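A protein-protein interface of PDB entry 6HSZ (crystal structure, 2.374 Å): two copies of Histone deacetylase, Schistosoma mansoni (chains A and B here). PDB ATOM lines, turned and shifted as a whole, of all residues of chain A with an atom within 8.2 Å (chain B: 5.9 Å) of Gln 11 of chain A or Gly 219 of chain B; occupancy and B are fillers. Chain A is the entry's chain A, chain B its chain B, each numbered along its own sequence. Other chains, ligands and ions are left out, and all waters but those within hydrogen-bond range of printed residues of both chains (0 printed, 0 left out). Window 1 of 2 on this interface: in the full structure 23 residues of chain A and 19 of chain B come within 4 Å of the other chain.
Gln 11 of chain A touches just these residues of chain B: Gly 219 (3.0 Å) and Thr 220 (3.9 Å). Gly 219 of chain B touches just one residue of chain A: Gln 11 (3.0 Å). Of chain A, only Gln 49 comes within 4 Å of Pro 218 of chain B. Thr 220 of chain B touches one residue of chain A. Of the printed residues of chain A, Phe 217 of chain B touches Gln 49. Of the printed residues of chain B, Gln 49 of chain A touches Phe 217 (3.5 Å) and Pro 218 (2.9 Å). The nearest residue of chain B that does not touch Gln 11 of chain A is Pro 218 of chain B (4.3 Å).
The side-chain amide nitrogen (NE2) of Gln 49 of chain A lies within hydrogen-bond range of the backbone carbonyl oxygen (O) of Pro 218 of chain B, at 2.9 Å. NE2 of Gln 11 of chain A is in hydrogen-bond range of O of Gly 219 of chain B (3.0 Å).
ND1 of His 190 of chain B lies within hydrogen-bond range of OG1 of Thr 220 of chain B, 2.5 Å away.
No position is printed for both chains.
Gln 11 of chain A touches Thr 220 of chain B (OE1 to CG2, 3.9 Å). Gln 49 of chain A touches Phe 217 of chain B (OE1 to CD2, 3.5 Å).
Hydrophobic or aromatic side chains of chain B within 4 Å of the printed part of chain A: Phe 217. Among the printed residues, 4 pairs touch across the chains.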
ATOM      1  N   TYR A   8       4.982 -17.182  -4.760  1.00  0.00           N
ATOM      2  CA  TYR A   8       5.592 -15.914  -4.373  1.00  0.00           C
ATOM      3  C   TYR A   8       5.740 -15.867  -2.862  1.00  0.00           C
ATOM      4  O   TYR A   8       5.355 -16.787  -2.140  1.00  0.00           O
ATOM      5  CB  TYR A   8       4.819 -14.691  -4.890  1.00  0.00           C
ATOM      6  CG  TYR A   8       3.461 -14.430  -4.292  1.00  0.00           C
ATOM      7  CD1 TYR A   8       2.314 -14.958  -4.883  1.00  0.00           C
ATOM      8  CD2 TYR A   8       3.306 -13.612  -3.167  1.00  0.00           C
ATOM      9  CE1 TYR A   8       1.039 -14.719  -4.352  1.00  0.00           C
ATOM     10  CE2 TYR A   8       2.022 -13.356  -2.624  1.00  0.00           C
ATOM     11  CZ  TYR A   8       0.895 -13.919  -3.226  1.00  0.00           C
ATOM     12  OH  TYR A   8      -0.376 -13.693  -2.720  1.00  0.00           O
ATOM     13  N   GLY A   9       6.328 -14.775  -2.398  1.00  0.00           N
ATOM     14  CA  GLY A   9       6.674 -14.591  -1.008  1.00  0.00           C
ATOM     15  C   GLY A   9       7.624 -13.422  -0.895  1.00  0.00           C
ATOM     16  O   GLY A   9       8.306 -13.079  -1.864  1.00  0.00           O
ATOM     17  N   ASP A  10       7.670 -12.777   0.264  1.00  0.00           N
ATOM     18  CA  ASP A  10       8.473 -11.569   0.368  1.00  0.00           C
ATOM     19  C   ASP A  10       9.953 -11.901   0.310  1.00  0.00           C
ATOM     20  O   ASP A  10      10.714 -11.266  -0.434  1.00  0.00           O
ATOM     21  CB  ASP A  10       8.111 -10.816   1.641  1.00  0.00           C
ATOM     22  CG  ASP A  10       6.774 -10.139   1.522  1.00  0.00           C
ATOM     23  OD1 ASP A  10       6.502  -9.590   0.431  1.00  0.00           O
ATOM     24  OD2 ASP A  10       5.989 -10.189   2.491  1.00  0.00           O
ATOM     25  N   GLN A  11      10.366 -12.917   1.074  1.00  0.00           N
ATOM     26  CA  GLN A  11      11.732 -13.422   0.992  1.00  0.00           C
ATOM     27  C   GLN A  11      12.042 -13.888  -0.422  1.00  0.00           C
ATOM     28  O   GLN A  11      13.078 -13.531  -0.996  1.00  0.00           O
ATOM     29  CB  GLN A  11      11.915 -14.563   1.991  1.00  0.00           C
ATOM     30  CG  GLN A  11      13.322 -15.093   2.105  1.00  0.00           C
ATOM     31  CD  GLN A  11      14.101 -14.429   3.229  1.00  0.00           C
ATOM     32  OE1 GLN A  11      13.902 -13.246   3.521  1.00  0.00           O
ATOM     33  NE2 GLN A  11      14.992 -15.190   3.867  1.00  0.00           N
ATOM     34  N   TYR A  12      11.133 -14.678  -1.001  1.00  0.00           N
ATOM     35  CA  TYR A  12      11.298 -15.164  -2.364  1.00  0.00           C
ATOM     36  C   TYR A  12      11.514 -14.008  -3.329  1.00  0.00           C
ATOM     37  O   TYR A  12      12.440 -14.021  -4.150  1.00  0.00           O
ATOM     38  CB  TYR A  12      10.062 -15.971  -2.755  1.00  0.00           C
ATOM     39  CG  TYR A  12      10.172 -16.768  -4.036  1.00  0.00           C
ATOM     40  CD1 TYR A  12      11.011 -17.870  -4.110  1.00  0.00           C
ATOM     41  CD2 TYR A  12       9.412 -16.454  -5.151  1.00  0.00           C
ATOM     42  CE1 TYR A  12      11.107 -18.635  -5.263  1.00  0.00           C
ATOM     43  CE2 TYR A  12       9.494 -17.214  -6.322  1.00  0.00           C
ATOM     44  CZ  TYR A  12      10.360 -18.307  -6.366  1.00  0.00           C
ATOM     45  OH  TYR A  12      10.488 -19.110  -7.482  1.00  0.00           O
ATOM     46  N   ARG A  13      10.673 -12.987  -3.231  1.00  0.00           N
ATOM     47  CA  ARG A  13      10.773 -11.865  -4.151  1.00  0.00           C
ATOM     48  C   ARG A  13      12.109 -11.144  -3.997  1.00  0.00           C
ATOM     49  O   ARG A  13      12.730 -10.752  -4.991  1.00  0.00           O
ATOM     50  CB  ARG A  13       9.591 -10.923  -3.916  1.00  0.00           C
ATOM     51  CG  ARG A  13       9.679  -9.562  -4.560  1.00  0.00           C
ATOM     52  CD  ARG A  13       8.573  -8.698  -4.022  1.00  0.00           C
ATOM     53  NE  ARG A  13       8.740  -7.327  -4.475  1.00  0.00           N
ATOM     54  CZ  ARG A  13       7.929  -6.696  -5.316  1.00  0.00           C
ATOM     55  NH1 ARG A  13       8.194  -5.442  -5.670  1.00  0.00           N
ATOM     56  NH2 ARG A  13       6.856  -7.310  -5.800  1.00  0.00           N
ATOM     57  N   GLN A  14      12.573 -10.974  -2.761  1.00  0.00           N
ATOM     58  CA  GLN A  14      13.847 -10.301  -2.533  1.00  0.00           C
ATOM     59  C   GLN A  14      15.017 -11.106  -3.117  1.00  0.00           C
ATOM     60  O   GLN A  14      15.893 -10.548  -3.793  1.00  0.00           O
ATOM     61  CB  GLN A  14      14.010 -10.058  -1.031  1.00  0.00           C
ATOM     62  CG  GLN A  14      15.231  -9.277  -0.608  1.00  0.00           C
ATOM     63  CD  GLN A  14      15.481  -9.377   0.901  1.00  0.00           C
ATOM     64  OE1 GLN A  14      14.737 -10.052   1.624  1.00  0.00           O
ATOM     65  NE2 GLN A  14      16.529  -8.708   1.377  1.00  0.00           N
ATOM     66  N   LEU A  15      15.013 -12.428  -2.914  1.00  0.00           N
ATOM     67  CA  LEU A  15      16.048 -13.301  -3.469  1.00  0.00           C
ATOM     68  C   LEU A  15      16.011 -13.342  -4.997  1.00  0.00           C
ATOM     69  O   LEU A  15      17.051 -13.227  -5.652  1.00  0.00           O
ATOM     70  CB  LEU A  15      15.882 -14.707  -2.900  1.00  0.00           C
ATOM     71  CG  LEU A  15      16.583 -14.856  -1.555  1.00  0.00           C
ATOM     72  CD1 LEU A  15      16.187 -16.131  -0.855  1.00  0.00           C
ATOM     73  CD2 LEU A  15      18.086 -14.801  -1.784  1.00  0.00           C
ATOM     74  N   CYS A  16      14.825 -13.532  -5.588  1.00  0.00           N
ATOM     75  CA  CYS A  16      14.720 -13.543  -7.044  1.00  0.00           C
ATOM     76  C   CYS A  16      15.110 -12.209  -7.690  1.00  0.00           C
ATOM     77  O   CYS A  16      15.420 -12.187  -8.886  1.00  0.00           O
ATOM     78  CB  CYS A  16      13.307 -13.912  -7.477  1.00  0.00           C
ATOM     79  SG  CYS A  16      12.816 -15.593  -7.103  1.00  0.00           S
ATOM     80  N   CYS A  17      15.115 -11.105  -6.946  1.00  0.00           N
ATOM     81  CA  CYS A  17      15.513  -9.817  -7.500  1.00  0.00           C
ATOM     82  C   CYS A  17      16.943  -9.439  -7.161  1.00  0.00           C
ATOM     83  O   CYS A  17      17.328  -8.285  -7.373  1.00  0.00           O
ATOM     84  CB  CYS A  17      14.578  -8.692  -7.023  1.00  0.00           C
ATOM     85  SG  CYS A  17      12.896  -8.824  -7.626  1.00  0.00           S
ATOM     86  N   SER A  18      17.743 -10.359  -6.632  1.00  0.00           N
ATOM     87  CA  SER A  18      19.069  -9.988  -6.159  1.00  0.00           C
ATOM     88  C   SER A  18      20.173 -10.276  -7.175  1.00  0.00           C
ATOM     89  O   SER A  18      21.351 -10.188  -6.825  1.00  0.00           O
ATOM     90  CB  SER A  18      19.371 -10.701  -4.842  1.00  0.00           C
ATOM     91  OG  SER A  18      19.515 -12.095  -5.061  1.00  0.00           O
ATOM     92  N   TYR A  26      11.557  -9.910 -11.700  1.00  0.00           N
ATOM     93  CA  TYR A  26      10.544 -10.671 -10.971  1.00  0.00           C
ATOM     94  C   TYR A  26       9.553  -9.752 -10.260  1.00  0.00           C
ATOM     95  O   TYR A  26       8.362 -10.076 -10.171  1.00  0.00           O
ATOM     96  CB  TYR A  26      11.200 -11.621  -9.964  1.00  0.00           C
ATOM     97  CG  TYR A  26      10.170 -12.420  -9.193  1.00  0.00           C
ATOM     98  CD1 TYR A  26       9.531 -13.519  -9.767  1.00  0.00           C
ATOM     99  CD2 TYR A  26       9.814 -12.063  -7.899  1.00  0.00           C
ATOM    100  CE1 TYR A  26       8.573 -14.244  -9.068  1.00  0.00           C
ATOM    101  CE2 TYR A  26       8.859 -12.782  -7.195  1.00  0.00           C
ATOM    102  CZ  TYR A  26       8.249 -13.871  -7.782  1.00  0.00           C
ATOM    103  OH  TYR A  26       7.296 -14.580  -7.081  1.00  0.00           O
ATOM    104  N   ARG A  44      -1.716 -18.824  -3.491  1.00  0.00           N
ATOM    105  CA  ARG A  44      -0.282 -18.585  -3.295  1.00  0.00           C
ATOM    106  C   ARG A  44       0.410 -19.862  -2.831  1.00  0.00           C
ATOM    107  O   ARG A  44       0.048 -20.416  -1.793  1.00  0.00           O
ATOM    108  CB  ARG A  44       0.011 -17.486  -2.279  1.00  0.00           C
ATOM    109  CG  ARG A  44       1.521 -17.503  -1.934  1.00  0.00           C
ATOM    110  CD  ARG A  44       1.991 -16.355  -1.067  1.00  0.00           C
ATOM    111  NE  ARG A  44       1.891 -16.639   0.362  1.00  0.00           N
ATOM    112  CZ  ARG A  44       2.899 -17.038   1.135  1.00  0.00           C
ATOM    113  NH1 ARG A  44       4.130 -17.216   0.646  1.00  0.00           N
ATOM    114  NH2 ARG A  44       2.669 -17.256   2.415  1.00  0.00           N
ATOM    115  N   PRO A  47       7.361 -20.941  -1.202  1.00  0.00           N
ATOM    116  CA  PRO A  47       8.566 -21.735  -1.522  1.00  0.00           C
ATOM    117  C   PRO A  47       8.905 -22.765  -0.442  1.00  0.00           C
ATOM    118  O   PRO A  47       8.724 -22.542   0.760  1.00  0.00           O
ATOM    119  CB  PRO A  47       9.661 -20.676  -1.670  1.00  0.00           C
ATOM    120  CG  PRO A  47       8.902 -19.372  -1.979  1.00  0.00           C
ATOM    121  CD  PRO A  47       7.596 -19.489  -1.226  1.00  0.00           C
ATOM    122  N   GLN A  49      10.821 -24.994   2.163  1.00  0.00           N
ATOM    123  CA  GLN A  49      11.961 -24.807   3.051  1.00  0.00           C
ATOM    124  C   GLN A  49      12.293 -26.142   3.706  1.00  0.00           C
ATOM    125  O   GLN A  49      11.441 -27.029   3.783  1.00  0.00           O
ATOM    126  CB  GLN A  49      11.693 -23.692   4.071  1.00  0.00           C
ATOM    127  CG  GLN A  49      11.628 -22.325   3.368  1.00  0.00           C
ATOM    128  CD  GLN A  49      11.104 -21.201   4.250  1.00  0.00           C
ATOM    129  OE1 GLN A  49       9.898 -21.120   4.531  1.00  0.00           O
ATOM    130  NE2 GLN A  49      12.009 -20.319   4.688  1.00  0.00           N
ATOM    131  N   ASP A 110      21.896 -18.314  -2.602  1.00  0.00           N
ATOM    132  CA  ASP A 110      20.513 -18.143  -2.157  1.00  0.00           C
ATOM    133  C   ASP A 110      19.581 -17.820  -3.328  1.00  0.00           C
ATOM    134  O   ASP A 110      18.444 -18.302  -3.376  1.00  0.00           O
ATOM    135  CB  ASP A 110      20.451 -17.063  -1.083  1.00  0.00           C
ATOM    136  CG  ASP A 110      21.218 -17.452   0.170  1.00  0.00           C
ATOM    137  OD1 ASP A 110      21.398 -18.664   0.413  1.00  0.00           O
ATOM    138  OD2 ASP A 110      21.658 -16.551   0.905  1.00  0.00           O
ATOM    139  N   ALA A 114      16.620 -20.399  -4.412  1.00  0.00           N
ATOM    140  CA  ALA A 114      15.235 -19.937  -4.299  1.00  0.00           C
ATOM    141  C   ALA A 114      14.374 -20.486  -5.429  1.00  0.00           C
ATOM    142  O   ALA A 114      13.240 -20.922  -5.192  1.00  0.00           O
ATOM    143  CB  ALA A 114      15.178 -18.407  -4.271  1.00  0.00           C
ATOM    144  N   GLN A 117      13.522 -23.874  -4.535  1.00  0.00           N
ATOM    145  CA  GLN A 117      12.484 -23.880  -3.507  1.00  0.00           C
ATOM    146  C   GLN A 117      11.109 -23.645  -4.115  1.00  0.00           C
ATOM    147  O   GLN A 117      10.126 -24.285  -3.724  1.00  0.00           O
ATOM    148  CB  GLN A 117      12.793 -22.820  -2.446  1.00  0.00           C
ATOM    149  CG  GLN A 117      14.135 -23.042  -1.737  1.00  0.00           C
ATOM    150  CD  GLN A 117      14.478 -21.937  -0.758  1.00  0.00           C
ATOM    151  OE1 GLN A 117      15.170 -20.983  -1.105  1.00  0.00           O
ATOM    152  NE2 GLN A 117      13.995 -22.063   0.479  1.00  0.00           N
ATOM    153  N   HIS B 190      14.799 -18.733  13.963  1.00  0.00           N
ATOM    154  CA  HIS B 190      14.654 -17.283  14.123  1.00  0.00           C
ATOM    155  C   HIS B 190      13.235 -16.897  14.529  1.00  0.00           C
ATOM    156  O   HIS B 190      12.261 -17.237  13.844  1.00  0.00           O
ATOM    157  CB  HIS B 190      15.001 -16.572  12.821  1.00  0.00           C
ATOM    158  CG  HIS B 190      14.788 -15.090  12.876  1.00  0.00           C
ATOM    159  ND1 HIS B 190      14.125 -14.389  11.890  1.00  0.00           N
ATOM    160  CD2 HIS B 190      15.175 -14.171  13.795  1.00  0.00           C
ATOM    161  CE1 HIS B 190      14.101 -13.104  12.208  1.00  0.00           C
ATOM    162  NE2 HIS B 190      14.729 -12.948  13.361  1.00  0.00           N
ATOM    163  N   ALA B 212      20.686 -20.520  11.066  1.00  0.00           N
ATOM    164  CA  ALA B 212      20.292 -19.938   9.790  1.00  0.00           C
ATOM    165  C   ALA B 212      21.301 -20.419   8.763  1.00  0.00           C
ATOM    166  O   ALA B 212      22.513 -20.401   9.009  1.00  0.00           O
ATOM    167  CB  ALA B 212      20.237 -18.404   9.824  1.00  0.00           C
ATOM    168  N   SER B 213      20.778 -20.891   7.645  1.00  0.00           N
ATOM    169  CA  SER B 213      21.544 -21.396   6.523  1.00  0.00           C
ATOM    170  C   SER B 213      20.622 -21.379   5.322  1.00  0.00           C
ATOM    171  O   SER B 213      19.402 -21.277   5.490  1.00  0.00           O
ATOM    172  CB  SER B 213      22.085 -22.821   6.807  1.00  0.00           C
ATOM    173  OG  SER B 213      21.059 -23.791   7.001  1.00  0.00           O
ATOM    174  N   PHE B 216      16.862 -22.970   5.106  1.00  0.00           N
ATOM    175  CA  PHE B 216      16.334 -23.333   6.416  1.00  0.00           C
ATOM    176  C   PHE B 216      15.309 -22.290   6.870  1.00  0.00           C
ATOM    177  O   PHE B 216      15.580 -21.082   6.836  1.00  0.00           O
ATOM    178  CB  PHE B 216      17.493 -23.452   7.414  1.00  0.00           C
ATOM    179  CG  PHE B 216      17.095 -23.894   8.795  1.00  0.00           C
ATOM    180  CD1 PHE B 216      16.913 -25.241   9.090  1.00  0.00           C
ATOM    181  CD2 PHE B 216      16.986 -22.970   9.821  1.00  0.00           C
ATOM    182  CE1 PHE B 216      16.583 -25.646  10.370  1.00  0.00           C
ATOM    183  CE2 PHE B 216      16.641 -23.372  11.099  1.00  0.00           C
ATOM    184  CZ  PHE B 216      16.443 -24.707  11.373  1.00  0.00           C
ATOM    185  N   PHE B 217      14.127 -22.764   7.263  1.00  0.00           N
ATOM    186  CA  PHE B 217      13.038 -21.962   7.842  1.00  0.00           C
ATOM    187  C   PHE B 217      13.475 -21.107   9.045  1.00  0.00           C
ATOM    188  O   PHE B 217      14.223 -21.567   9.903  1.00  0.00           O
ATOM    189  CB  PHE B 217      11.900 -22.921   8.258  1.00  0.00           C
ATOM    190  CG  PHE B 217      10.631 -22.242   8.716  1.00  0.00           C
ATOM    191  CD1 PHE B 217      10.481 -21.825  10.038  1.00  0.00           C
ATOM    192  CD2 PHE B 217       9.570 -22.080   7.843  1.00  0.00           C
ATOM    193  CE1 PHE B 217       9.323 -21.223  10.463  1.00  0.00           C
ATOM    194  CE2 PHE B 217       8.399 -21.483   8.258  1.00  0.00           C
ATOM    195  CZ  PHE B 217       8.277 -21.047   9.574  1.00  0.00           C
ATOM    196  N   PRO B 218      13.006 -19.852   9.112  1.00  0.00           N
ATOM    197  CA  PRO B 218      12.207 -19.199   8.078  1.00  0.00           C
ATOM    198  C   PRO B 218      13.056 -18.384   7.106  1.00  0.00           C
ATOM    199  O   PRO B 218      12.536 -17.888   6.114  1.00  0.00           O
ATOM    200  CB  PRO B 218      11.268 -18.304   8.890  1.00  0.00           C
ATOM    201  CG  PRO B 218      12.070 -17.917  10.076  1.00  0.00           C
ATOM    202  CD  PRO B 218      13.052 -19.058  10.351  1.00  0.00           C
ATOM    203  N   GLY B 219      14.350 -18.243   7.371  1.00  0.00           N
ATOM    204  CA  GLY B 219      15.243 -17.560   6.442  1.00  0.00           C
ATOM    205  C   GLY B 219      15.731 -16.197   6.887  1.00  0.00           C
ATOM    206  O   GLY B 219      16.688 -15.678   6.298  1.00  0.00           O
ATOM    207  N   THR B 220      15.123 -15.598   7.894  1.00  0.00           N
ATOM    208  CA  THR B 220      15.517 -14.292   8.376  1.00  0.00           C
ATOM    209  C   THR B 220      16.433 -14.468   9.584  1.00  0.00           C
ATOM    210  O   THR B 220      16.830 -15.585   9.922  1.00  0.00           O
ATOM    211  CB  THR B 220      14.267 -13.479   8.696  1.00  0.00           C
ATOM    212  OG1 THR B 220      13.364 -14.296   9.459  1.00  0.00           O
ATOM    213  CG2 THR B 220      13.586 -13.022   7.407  1.00  0.00           C
ATOM    214  N   GLY B 221      16.773 -13.364  10.250  1.00  0.00           N
ATOM    215  CA  GLY B 221      17.683 -13.429  11.387  1.00  0.00           C
ATOM    216  C   GLY B 221      19.147 -13.610  11.026  1.00  0.00           C
ATOM    217  O   GLY B 221      19.917 -14.162  11.824  1.00  0.00           O
ATOM    218  N   THR B 222      19.562 -13.159   9.846  1.00  0.00           N
ATOM    219  CA  THR B 222      20.942 -13.300   9.384  1.00  0.00           C
ATOM    220  C   THR B 222      21.229 -12.212   8.343  1.00  0.00           C
ATOM    221  O   THR B 222      20.405 -11.321   8.107  1.00  0.00           O
ATOM    222  CB  THR B 222      21.172 -14.711   8.836  1.00  0.00           C
ATOM    223  OG1 THR B 222      22.547 -14.870   8.477  1.00  0.00           O
ATOM    224  CG2 THR B 222      20.301 -14.952   7.613  1.00  0.00           C
ATOM    225  N   TRP B 223      22.389 -12.302   7.700  1.00  0.00           N
ATOM    226  CA  TRP B 223      22.854 -11.276   6.770  1.00  0.00           C
ATOM    227  C   TRP B 223      21.853 -11.035   5.634  1.00  0.00           C
ATOM    228  O   TRP B 223      21.083 -11.916   5.244  1.00  0.00           O
ATOM    229  CB  TRP B 223      24.204 -11.680   6.177  1.00  0.00           C
ATOM    230  CG  TRP B 223      25.300 -11.803   7.182  1.00  0.00           C
ATOM    231  CD1 TRP B 223      25.783 -12.959   7.746  1.00  0.00           C
ATOM    232  CD2 TRP B 223      26.053 -10.732   7.757  1.00  0.00           C
ATOM    233  NE1 TRP B 223      26.801 -12.673   8.627  1.00  0.00           N
ATOM    234  CE2 TRP B 223      26.989 -11.314   8.657  1.00  0.00           C
ATOM    235  CE3 TRP B 223      26.044  -9.344   7.590  1.00  0.00           C
ATOM    236  CZ2 TRP B 223      27.901 -10.544   9.399  1.00  0.00           C
ATOM    237  CZ3 TRP B 223      26.946  -8.580   8.324  1.00  0.00           C
ATOM    238  CH2 TRP B 223      27.862  -9.182   9.222  1.00  0.00           C
